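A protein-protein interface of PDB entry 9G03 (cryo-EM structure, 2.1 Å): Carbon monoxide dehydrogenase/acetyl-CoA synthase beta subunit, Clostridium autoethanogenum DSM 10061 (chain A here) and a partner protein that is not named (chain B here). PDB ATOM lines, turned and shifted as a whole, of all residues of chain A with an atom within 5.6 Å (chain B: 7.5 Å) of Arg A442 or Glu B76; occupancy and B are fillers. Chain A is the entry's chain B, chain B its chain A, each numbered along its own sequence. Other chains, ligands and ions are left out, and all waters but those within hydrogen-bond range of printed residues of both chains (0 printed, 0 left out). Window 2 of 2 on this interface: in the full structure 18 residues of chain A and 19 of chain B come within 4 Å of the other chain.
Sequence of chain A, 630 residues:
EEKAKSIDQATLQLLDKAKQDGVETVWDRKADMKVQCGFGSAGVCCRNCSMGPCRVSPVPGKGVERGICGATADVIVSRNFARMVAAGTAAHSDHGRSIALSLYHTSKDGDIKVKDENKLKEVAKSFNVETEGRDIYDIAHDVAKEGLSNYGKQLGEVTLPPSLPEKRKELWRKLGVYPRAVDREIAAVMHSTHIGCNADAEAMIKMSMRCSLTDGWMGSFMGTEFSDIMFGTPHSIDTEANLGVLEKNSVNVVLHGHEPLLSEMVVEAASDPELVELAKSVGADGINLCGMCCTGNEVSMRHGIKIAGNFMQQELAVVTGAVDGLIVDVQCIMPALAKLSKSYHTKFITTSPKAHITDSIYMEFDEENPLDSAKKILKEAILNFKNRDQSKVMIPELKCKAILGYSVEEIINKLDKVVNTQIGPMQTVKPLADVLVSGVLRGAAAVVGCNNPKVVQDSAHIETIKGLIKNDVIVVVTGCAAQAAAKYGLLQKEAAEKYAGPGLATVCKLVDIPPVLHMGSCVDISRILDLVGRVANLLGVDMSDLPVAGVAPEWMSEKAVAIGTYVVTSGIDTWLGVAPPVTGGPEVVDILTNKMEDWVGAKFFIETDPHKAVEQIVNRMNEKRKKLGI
Ser A438 touches Leu B3 (O to CB, 3.8 Å).
O of Ser A438 touches CE1 of Phe B4 (3.4 Å).
Gly A439 touches Phe B4 (O to CE1, 3.4 Å).
Asp A472 touches Met B77.
Printed residues of chain B within 4 Å of Arg A442: Glu B76 (2.9 Å).
Printed residues of chain A within 4 Å of Glu B76: Arg A442.
Printed residues of chain B within 4 Å of Ile A630: Asn B2 (3.3 Å).
Of the printed residues of chain A, Leu B3 touches Ser A438.
Of the printed residues of chain A, Asn B2 touches Ile A630.
Printed residues of chain B within 4 Å of Ser A438: Leu B3 and Phe B4.
The nearest residue of chain A that does not touch Glu B76 is Lys A626 (4.5 Å).
The nearest printed residue of chain B that does not touch Ile A630 is Glu B76 (4.7 Å).
The side-chain amide nitrogen (ND2) of Asn B2 sits close to the backbone carbonyl oxygen (O) of Ile A630, at 3.3 Å.
The side-chain carboxylate of Glu B76 is in salt-bridge range of the guanidinium group of Arg A442 (2.9 Å).
The side-chain amide oxygen of Asn B2 sits at hydrogen-bond distance from the backbone NH of Phe B4, 3.2 Å away.
N of Gln B5 is in hydrogen-bond range of OD1 of Asn B2 (2.8 Å).
OE1 of Gln B5 sits close to OE2 of Glu B76.
The backbone NH (N) of Arg A442 is in hydrogen-bond range of the backbone carbonyl oxygen (O) of Asp A472, 2.9 Å away.
The guanidinium group of Arg A442 lies within hydrogen-bond range of the side-chain amide oxygen of Asn A622 (3.1 Å).
The backbone carbonyl oxygen of Arg A442 lies within hydrogen-bond range of the guanidinium group of Arg A625 (3.3 Å).
Hydrophobic or aromatic side chains of chain B within 4 Å of the printed part of chain A: Leu B3, Phe B4 and Met B77.
Along chain B the printed residues that touch a printed residue of chain A span positions 2 to 77.
Among the printed residues, 6 pairs touch across the chains.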
ATOM      1  N   LEU A 436      11.613  12.798  -0.288  1.00  0.00           N
ATOM      2  CA  LEU A 436      12.929  13.177  -0.797  1.00  0.00           C
ATOM      3  C   LEU A 436      13.212  12.523  -2.144  1.00  0.00           C
ATOM      4  O   LEU A 436      13.737  13.173  -3.049  1.00  0.00           O
ATOM      5  CB  LEU A 436      14.011  12.813   0.218  1.00  0.00           C
ATOM      6  CG  LEU A 436      14.039  13.672   1.484  1.00  0.00           C
ATOM      7  CD1 LEU A 436      15.045  13.128   2.480  1.00  0.00           C
ATOM      8  CD2 LEU A 436      14.352  15.124   1.153  1.00  0.00           C
ATOM      9  N   SER A 438      11.028  11.323  -4.403  1.00  0.00           N
ATOM     10  CA  SER A 438      10.144  11.797  -5.464  1.00  0.00           C
ATOM     11  C   SER A 438      10.499  13.202  -5.936  1.00  0.00           C
ATOM     12  O   SER A 438      10.140  13.570  -7.055  1.00  0.00           O
ATOM     13  CB  SER A 438       8.680  11.763  -5.006  1.00  0.00           C
ATOM     14  OG  SER A 438       8.408  12.789  -4.071  1.00  0.00           O
ATOM     15  N   GLY A 439      11.208  13.985  -5.129  1.00  0.00           N
ATOM     16  CA  GLY A 439      11.520  15.345  -5.500  1.00  0.00           C
ATOM     17  C   GLY A 439      10.528  16.381  -5.023  1.00  0.00           C
ATOM     18  O   GLY A 439      10.746  17.571  -5.263  1.00  0.00           O
ATOM     19  N   VAL A 440       9.476  15.980  -4.309  1.00  0.00           N
ATOM     20  CA  VAL A 440       8.578  16.958  -3.706  1.00  0.00           C
ATOM     21  C   VAL A 440       9.356  17.833  -2.733  1.00  0.00           C
ATOM     22  O   VAL A 440       9.181  19.054  -2.696  1.00  0.00           O
ATOM     23  CB  VAL A 440       7.388  16.245  -3.031  1.00  0.00           C
ATOM     24  CG1 VAL A 440       6.517  17.223  -2.262  1.00  0.00           C
ATOM     25  CG2 VAL A 440       6.553  15.525  -4.076  1.00  0.00           C
ATOM     26  N   LEU A 441      10.235  17.223  -1.954  1.00  0.00           N
ATOM     27  CA  LEU A 441      11.241  17.940  -1.192  1.00  0.00           C
ATOM     28  C   LEU A 441      12.571  17.777  -1.912  1.00  0.00           C
ATOM     29  O   LEU A 441      12.960  16.659  -2.260  1.00  0.00           O
ATOM     30  CB  LEU A 441      11.351  17.432   0.246  1.00  0.00           C
ATOM     31  CG  LEU A 441      10.192  17.728   1.183  1.00  0.00           C
ATOM     32  CD1 LEU A 441      10.566  17.266   2.589  1.00  0.00           C
ATOM     33  CD2 LEU A 441       9.806  19.207   1.148  1.00  0.00           C
ATOM     34  N   ARG A 442      13.253  18.899  -2.144  1.00  0.00           N
ATOM     35  CA  ARG A 442      14.543  18.861  -2.819  1.00  0.00           C
ATOM     36  C   ARG A 442      15.629  18.300  -1.913  1.00  0.00           C
ATOM     37  O   ARG A 442      16.564  17.666  -2.403  1.00  0.00           O
ATOM     38  CB  ARG A 442      14.916  20.264  -3.301  1.00  0.00           C
ATOM     39  CG  ARG A 442      13.822  20.951  -4.132  1.00  0.00           C
ATOM     40  CD  ARG A 442      13.295  20.065  -5.269  1.00  0.00           C
ATOM     41  NE  ARG A 442      14.339  19.762  -6.242  1.00  0.00           N
ATOM     42  CZ  ARG A 442      14.301  18.765  -7.116  1.00  0.00           C
ATOM     43  NH1 ARG A 442      13.273  17.940  -7.186  1.00  0.00           N
ATOM     44  NH2 ARG A 442      15.326  18.591  -7.942  1.00  0.00           N
ATOM     45  N   GLY A 443      15.519  18.507  -0.607  1.00  0.00           N
ATOM     46  CA  GLY A 443      16.498  17.970   0.313  1.00  0.00           C
ATOM     47  C   GLY A 443      16.213  18.399   1.735  1.00  0.00           C
ATOM     48  O   GLY A 443      15.177  19.001   2.039  1.00  0.00           O
ATOM     49  N   ALA A 444      17.151  18.066   2.608  1.00  0.00           N
ATOM     50  CA  ALA A 444      17.091  18.445   4.010  1.00  0.00           C
ATOM     51  C   ALA A 444      18.396  19.108   4.413  1.00  0.00           C
ATOM     52  O   ALA A 444      19.478  18.649   4.043  1.00  0.00           O
ATOM     53  CB  ALA A 444      16.814  17.241   4.914  1.00  0.00           C
ATOM     54  N   ASN A 471      13.216  27.243  -1.204  1.00  0.00           N
ATOM     55  CA  ASN A 471      13.636  26.321  -2.253  1.00  0.00           C
ATOM     56  C   ASN A 471      13.199  24.878  -1.996  1.00  0.00           C
ATOM     57  O   ASN A 471      13.818  23.950  -2.524  1.00  0.00           O
ATOM     58  CB  ASN A 471      15.156  26.375  -2.414  1.00  0.00           C
ATOM     59  CG  ASN A 471      15.620  27.646  -3.070  1.00  0.00           C
ATOM     60  OD1 ASN A 471      15.584  27.761  -4.288  1.00  0.00           O
ATOM     61  ND2 ASN A 471      16.060  28.612  -2.273  1.00  0.00           N
ATOM     62  N   ASP A 472      12.148  24.675  -1.206  1.00  0.00           N
ATOM     63  CA  ASP A 472      11.616  23.348  -0.879  1.00  0.00           C
ATOM     64  C   ASP A 472      12.691  22.443  -0.280  1.00  0.00           C
ATOM     65  O   ASP A 472      12.761  21.253  -0.575  1.00  0.00           O
ATOM     66  CB  ASP A 472      10.969  22.685  -2.100  1.00  0.00           C
ATOM     67  CG  ASP A 472       9.557  23.184  -2.354  1.00  0.00           C
ATOM     68  OD1 ASP A 472       8.945  23.732  -1.419  1.00  0.00           O
ATOM     69  OD2 ASP A 472       9.052  23.026  -3.485  1.00  0.00           O
ATOM     70  N   VAL A 473      13.531  23.010   0.576  1.00  0.00           N
ATOM     71  CA  VAL A 473      14.459  22.244   1.392  1.00  0.00           C
ATOM     72  C   VAL A 473      13.954  22.319   2.822  1.00  0.00           C
ATOM     73  O   VAL A 473      13.892  23.408   3.410  1.00  0.00           O
ATOM     74  CB  VAL A 473      15.903  22.760   1.296  1.00  0.00           C
ATOM     75  CG1 VAL A 473      16.825  21.941   2.211  1.00  0.00           C
ATOM     76  CG2 VAL A 473      16.398  22.715  -0.142  1.00  0.00           C
ATOM     77  N   PRO A 547      20.771  14.053  -0.820  1.00  0.00           N
ATOM     78  CA  PRO A 547      20.751  15.528  -0.963  1.00  0.00           C
ATOM     79  C   PRO A 547      20.533  16.220   0.380  1.00  0.00           C
ATOM     80  O   PRO A 547      19.487  16.787   0.677  1.00  0.00           O
ATOM     81  CB  PRO A 547      19.597  15.746  -1.949  1.00  0.00           C
ATOM     82  CG  PRO A 547      18.640  14.610  -1.657  1.00  0.00           C
ATOM     83  CD  PRO A 547      19.498  13.436  -1.234  1.00  0.00           C
ATOM     84  N   MET A 621      22.863  20.016  -3.839  1.00  0.00           N
ATOM     85  CA  MET A 621      21.808  19.025  -3.640  1.00  0.00           C
ATOM     86  C   MET A 621      21.283  18.511  -4.975  1.00  0.00           C
ATOM     87  O   MET A 621      21.064  17.310  -5.135  1.00  0.00           O
ATOM     88  CB  MET A 621      20.671  19.613  -2.807  1.00  0.00           C
ATOM     89  CG  MET A 621      20.994  19.712  -1.334  1.00  0.00           C
ATOM     90  SD  MET A 621      19.680  20.462  -0.359  1.00  0.00           S
ATOM     91  CE  MET A 621      20.278  20.160   1.306  1.00  0.00           C
ATOM     92  N   ASN A 622      21.105  19.394  -5.951  1.00  0.00           N
ATOM     93  CA  ASN A 622      20.610  18.948  -7.248  1.00  0.00           C
ATOM     94  C   ASN A 622      21.618  18.024  -7.926  1.00  0.00           C
ATOM     95  O   ASN A 622      21.234  17.009  -8.516  1.00  0.00           O
ATOM     96  CB  ASN A 622      20.283  20.146  -8.135  1.00  0.00           C
ATOM     97  CG  ASN A 622      18.959  20.797  -7.765  1.00  0.00           C
ATOM     98  OD1 ASN A 622      17.969  20.119  -7.525  1.00  0.00           O
ATOM     99  ND2 ASN A 622      18.950  22.117  -7.696  1.00  0.00           N
ATOM    100  N   ARG A 625      21.443  14.700  -6.295  1.00  0.00           N
ATOM    101  CA  ARG A 625      20.233  14.018  -6.750  1.00  0.00           C
ATOM    102  C   ARG A 625      20.435  13.404  -8.132  1.00  0.00           C
ATOM    103  O   ARG A 625      20.040  12.261  -8.374  1.00  0.00           O
ATOM    104  CB  ARG A 625      19.051  14.992  -6.788  1.00  0.00           C
ATOM    105  CG  ARG A 625      18.568  15.490  -5.434  1.00  0.00           C
ATOM    106  CD  ARG A 625      17.350  16.396  -5.573  1.00  0.00           C
ATOM    107  NE  ARG A 625      16.204  15.662  -6.089  1.00  0.00           N
ATOM    108  CZ  ARG A 625      15.353  14.973  -5.338  1.00  0.00           C
ATOM    109  NH1 ARG A 625      15.421  14.988  -4.017  1.00  0.00           N
ATOM    110  NH2 ARG A 625      14.426  14.230  -5.930  1.00  0.00           N
ATOM    111  N   LYS A 626      21.050  14.151  -9.053  1.00  0.00           N
ATOM    112  CA  LYS A 626      21.287  13.611 -10.390  1.00  0.00           C
ATOM    113  C   LYS A 626      22.248  12.433 -10.350  1.00  0.00           C
ATOM    114  O   LYS A 626      22.096  11.471 -11.107  1.00  0.00           O
ATOM    115  CB  LYS A 626      21.818  14.701 -11.320  1.00  0.00           C
ATOM    116  CG  LYS A 626      20.741  15.662 -11.792  1.00  0.00           C
ATOM    117  CD  LYS A 626      21.194  17.116 -11.758  1.00  0.00           C
ATOM    118  CE  LYS A 626      20.013  18.065 -11.588  1.00  0.00           C
ATOM    119  NZ  LYS A 626      19.203  17.790 -10.354  1.00  0.00           N
ATOM    120  N   ILE A 630      17.536  10.465  -8.673  1.00  0.00           N
ATOM    121  CA  ILE A 630      16.228  10.955  -8.247  1.00  0.00           C
ATOM    122  C   ILE A 630      16.002  12.379  -8.743  1.00  0.00           C
ATOM    123  O   ILE A 630      14.989  13.004  -8.425  1.00  0.00           O
ATOM    124  CB  ILE A 630      16.090  10.878  -6.719  1.00  0.00           C
ATOM    125  CG1 ILE A 630      17.157  11.755  -6.045  1.00  0.00           C
ATOM    126  CG2 ILE A 630      16.196   9.433  -6.261  1.00  0.00           C
ATOM    127  CD1 ILE A 630      17.069  11.805  -4.539  1.00  0.00           C
ATOM    128  N   ASN B   2      13.609  10.381 -13.188  1.00  0.00           N
ATOM    129  CA  ASN B   2      12.885  10.579 -11.948  1.00  0.00           C
ATOM    130  C   ASN B   2      11.429  10.951 -12.243  1.00  0.00           C
ATOM    131  O   ASN B   2      10.993  11.014 -13.394  1.00  0.00           O
ATOM    132  CB  ASN B   2      13.593  11.637 -11.105  1.00  0.00           C
ATOM    133  CG  ASN B   2      13.728  12.961 -11.821  1.00  0.00           C
ATOM    134  OD1 ASN B   2      12.801  13.420 -12.477  1.00  0.00           O
ATOM    135  ND2 ASN B   2      14.886  13.581 -11.695  1.00  0.00           N
ATOM    136  N   LEU B   3      10.664  11.197 -11.176  1.00  0.00           N
ATOM    137  CA  LEU B   3       9.237  11.473 -11.316  1.00  0.00           C
ATOM    138  C   LEU B   3       8.976  12.729 -12.139  1.00  0.00           C
ATOM    139  O   LEU B   3       8.128  12.729 -13.037  1.00  0.00           O
ATOM    140  CB  LEU B   3       8.594  11.605  -9.934  1.00  0.00           C
ATOM    141  CG  LEU B   3       7.087  11.886  -9.926  1.00  0.00           C
ATOM    142  CD1 LEU B   3       6.299  10.752 -10.559  1.00  0.00           C
ATOM    143  CD2 LEU B   3       6.604  12.150  -8.506  1.00  0.00           C
ATOM    144  N   PHE B   4       9.698  13.812 -11.846  1.00  0.00           N
ATOM    145  CA  PHE B   4       9.494  15.060 -12.573  1.00  0.00           C
ATOM    146  C   PHE B   4       9.791  14.882 -14.052  1.00  0.00           C
ATOM    147  O   PHE B   4       9.022  15.327 -14.910  1.00  0.00           O
ATOM    148  CB  PHE B   4      10.372  16.175 -11.994  1.00  0.00           C
ATOM    149  CG  PHE B   4       9.862  16.754 -10.712  1.00  0.00           C
ATOM    150  CD1 PHE B   4      10.123  16.129  -9.509  1.00  0.00           C
ATOM    151  CD2 PHE B   4       9.137  17.932 -10.703  1.00  0.00           C
ATOM    152  CE1 PHE B   4       9.657  16.651  -8.326  1.00  0.00           C
ATOM    153  CE2 PHE B   4       8.678  18.465  -9.520  1.00  0.00           C
ATOM    154  CZ  PHE B   4       8.934  17.823  -8.327  1.00  0.00           C
ATOM    155  N   GLN B   5      10.897  14.220 -14.369  1.00  0.00           N
ATOM    156  CA  GLN B   5      11.262  14.015 -15.763  1.00  0.00           C
ATOM    157  C   GLN B   5      10.272  13.095 -16.455  1.00  0.00           C
ATOM    158  O   GLN B   5       9.932  13.314 -17.620  1.00  0.00           O
ATOM    159  CB  GLN B   5      12.682  13.456 -15.860  1.00  0.00           C
ATOM    160  CG  GLN B   5      13.755  14.429 -15.405  1.00  0.00           C
ATOM    161  CD  GLN B   5      13.646  15.774 -16.086  1.00  0.00           C
ATOM    162  OE1 GLN B   5      13.649  16.814 -15.431  1.00  0.00           O
ATOM    163  NE2 GLN B   5      13.538  15.761 -17.408  1.00  0.00           N
ATOM    164  N   THR B   6       9.780  12.078 -15.753  1.00  0.00           N
ATOM    165  CA  THR B   6       8.762  11.218 -16.343  1.00  0.00           C
ATOM    166  C   THR B   6       7.504  12.014 -16.676  1.00  0.00           C
ATOM    167  O   THR B   6       6.938  11.862 -17.763  1.00  0.00           O
ATOM    168  CB  THR B   6       8.429  10.066 -15.396  1.00  0.00           C
ATOM    169  OG1 THR B   6       9.631   9.371 -15.049  1.00  0.00           O
ATOM    170  CG2 THR B   6       7.457   9.087 -16.046  1.00  0.00           C
ATOM    171  N   PHE B   8       7.236  15.301 -17.193  1.00  0.00           N
ATOM    172  CA  PHE B   8       7.516  16.228 -18.285  1.00  0.00           C
ATOM    173  C   PHE B   8       7.556  15.507 -19.631  1.00  0.00           C
ATOM    174  O   PHE B   8       7.020  16.008 -20.626  1.00  0.00           O
ATOM    175  CB  PHE B   8       8.836  16.962 -18.019  1.00  0.00           C
ATOM    176  CG  PHE B   8       8.802  17.892 -16.823  1.00  0.00           C
ATOM    177  CD1 PHE B   8       7.632  18.527 -16.451  1.00  0.00           C
ATOM    178  CD2 PHE B   8       9.944  18.120 -16.069  1.00  0.00           C
ATOM    179  CE1 PHE B   8       7.594  19.373 -15.361  1.00  0.00           C
ATOM    180  CE2 PHE B   8       9.911  18.974 -14.969  1.00  0.00           C
ATOM    181  CZ  PHE B   8       8.731  19.598 -14.621  1.00  0.00           C
ATOM    182  N   VAL B  73       6.492  23.771 -17.869  1.00  0.00           N
ATOM    183  CA  VAL B  73       7.735  24.431 -17.488  1.00  0.00           C
ATOM    184  C   VAL B  73       8.595  23.381 -16.800  1.00  0.00           C
ATOM    185  O   VAL B  73       8.231  22.884 -15.728  1.00  0.00           O
ATOM    186  CB  VAL B  73       7.489  25.637 -16.568  1.00  0.00           C
ATOM    187  CG1 VAL B  73       8.800  26.303 -16.196  1.00  0.00           C
ATOM    188  CG2 VAL B  73       6.556  26.631 -17.234  1.00  0.00           C
ATOM    189  N   GLU B  74       9.728  23.044 -17.411  1.00  0.00           N
ATOM    190  CA  GLU B  74      10.547  21.919 -16.956  1.00  0.00           C
ATOM    191  C   GLU B  74      11.514  22.366 -15.860  1.00  0.00           C
ATOM    192  O   GLU B  74      12.727  22.462 -16.044  1.00  0.00           O
ATOM    193  CB  GLU B  74      11.283  21.295 -18.129  1.00  0.00           C
ATOM    194  CG  GLU B  74      10.356  20.754 -19.196  1.00  0.00           C
ATOM    195  CD  GLU B  74      10.998  19.684 -20.043  1.00  0.00           C
ATOM    196  OE1 GLU B  74      11.902  18.982 -19.546  1.00  0.00           O
ATOM    197  OE2 GLU B  74      10.597  19.547 -21.215  1.00  0.00           O
ATOM    198  N   GLU B  75      10.942  22.625 -14.689  1.00  0.00           N
ATOM    199  CA  GLU B  75      11.704  22.911 -13.483  1.00  0.00           C
ATOM    200  C   GLU B  75      11.185  22.008 -12.375  1.00  0.00           C
ATOM    201  O   GLU B  75       9.972  21.893 -12.186  1.00  0.00           O
ATOM    202  CB  GLU B  75      11.585  24.387 -13.097  1.00  0.00           C
ATOM    203  CG  GLU B  75      12.316  25.315 -14.059  1.00  0.00           C
ATOM    204  CD  GLU B  75      11.757  26.722 -14.075  1.00  0.00           C
ATOM    205  OE1 GLU B  75      10.910  27.046 -13.218  1.00  0.00           O
ATOM    206  OE2 GLU B  75      12.165  27.508 -14.953  1.00  0.00           O
ATOM    207  N   GLU B  76      12.104  21.348 -11.668  1.00  0.00           N
ATOM    208  CA  GLU B  76      11.743  20.292 -10.722  1.00  0.00           C
ATOM    209  C   GLU B  76      11.264  20.898  -9.401  1.00  0.00           C
ATOM    210  O   GLU B  76      11.949  20.889  -8.377  1.00  0.00           O
ATOM    211  CB  GLU B  76      12.906  19.330 -10.522  1.00  0.00           C
ATOM    212  CG  GLU B  76      13.313  18.626 -11.807  1.00  0.00           C
ATOM    213  CD  GLU B  76      14.200  17.416 -11.579  1.00  0.00           C
ATOM    214  OE1 GLU B  76      14.691  17.231 -10.449  1.00  0.00           O
ATOM    215  OE2 GLU B  76      14.404  16.648 -12.539  1.00  0.00           O
ATOM    216  N   MET B  77      10.063  21.460  -9.455  1.00  0.00           N
ATOM    217  CA  MET B  77       9.336  21.915  -8.280  1.00  0.00           C
ATOM    218  C   MET B  77       7.899  21.432  -8.411  1.00  0.00           C
ATOM    219  O   MET B  77       7.391  21.253  -9.520  1.00  0.00           O
ATOM    220  CB  MET B  77       9.377  23.443  -8.113  1.00  0.00           C
ATOM    221  CG  MET B  77      10.774  24.037  -8.037  1.00  0.00           C
ATOM    222  SD  MET B  77      11.660  23.733  -6.491  1.00  0.00           S
ATOM    223  CE  MET B  77      11.018  25.048  -5.458  1.00  0.00           C
ATOM    224  N   LEU B  78       7.242  21.244  -7.271  1.00  0.00           N
ATOM    225  CA  LEU B  78       5.950  20.564  -7.251  1.00  0.00           C
ATOM    226  C   LEU B  78       4.901  21.303  -8.082  1.00  0.00           C
ATOM    227  O   LEU B  78       4.086  20.675  -8.768  1.00  0.00           O
ATOM    228  CB  LEU B  78       5.474  20.394  -5.816  1.00  0.00           C
ATOM    229  CG  LEU B  78       4.138  19.669  -5.653  1.00  0.00           C
ATOM    230  CD1 LEU B  78       4.206  18.247  -6.177  1.00  0.00           C
ATOM    231  CD2 LEU B  78       3.724  19.681  -4.197  1.00  0.00           C
ATOM    232  N   ASP B  79       4.888  22.634  -8.012  1.00  0.00           N
ATOM    233  CA  ASP B  79       3.902  23.397  -8.772  1.00  0.00           C
ATOM    234  C   ASP B  79       4.055  23.164 -10.272  1.00  0.00           C
ATOM    235  O   ASP B  79       3.058  23.021 -10.986  1.00  0.00           O
ATOM    236  CB  ASP B  79       4.008  24.885  -8.434  1.00  0.00           C
ATOM    237  CG  ASP B  79       5.400  25.445  -8.650  1.00  0.00           C
ATOM    238  OD1 ASP B  79       6.381  24.805  -8.225  1.00  0.00           O
ATOM    239  OD2 ASP B  79       5.510  26.533  -9.248  1.00  0.00           O
ATOM    240  N   LYS B  80       5.294  23.108 -10.769  1.00  0.00           N
ATOM    241  CA  LYS B  80       5.509  22.828 -12.187  1.00  0.00           C
ATOM    242  C   LYS B  80       5.037  21.426 -12.552  1.00  0.00           C
ATOM    243  O   LYS B  80       4.519  21.210 -13.650  1.00  0.00           O
ATOM    244  CB  LYS B  80       6.981  23.008 -12.557  1.00  0.00           C
ATOM    245  CG  LYS B  80       7.426  24.458 -12.664  1.00  0.00           C
ATOM    246  CD  LYS B  80       7.838  25.024 -11.320  1.00  0.00           C
ATOM    247  CE  LYS B  80       8.148  26.505 -11.403  1.00  0.00           C
ATOM    248  NZ  LYS B  80       6.953  27.311 -11.752  1.00  0.00           N
ATOM    249  N   LEU B  81       5.234  20.456 -11.661  1.00  0.00           N
ATOM    250  CA  LEU B  81       4.750  19.105 -11.923  1.00  0.00           C
ATOM    251  C   LEU B  81       3.225  19.082 -12.026  1.00  0.00           C
ATOM    252  O   LEU B  81       2.661  18.437 -12.920  1.00  0.00           O
ATOM    253  CB  LEU B  81       5.250  18.160 -10.828  1.00  0.00           C
ATOM    254  CG  LEU B  81       4.923  16.666 -10.931  1.00  0.00           C
ATOM    255  CD1 LEU B  81       6.032  15.839 -10.317  1.00  0.00           C
ATOM    256  CD2 LEU B  81       3.601  16.333 -10.253  1.00  0.00           C
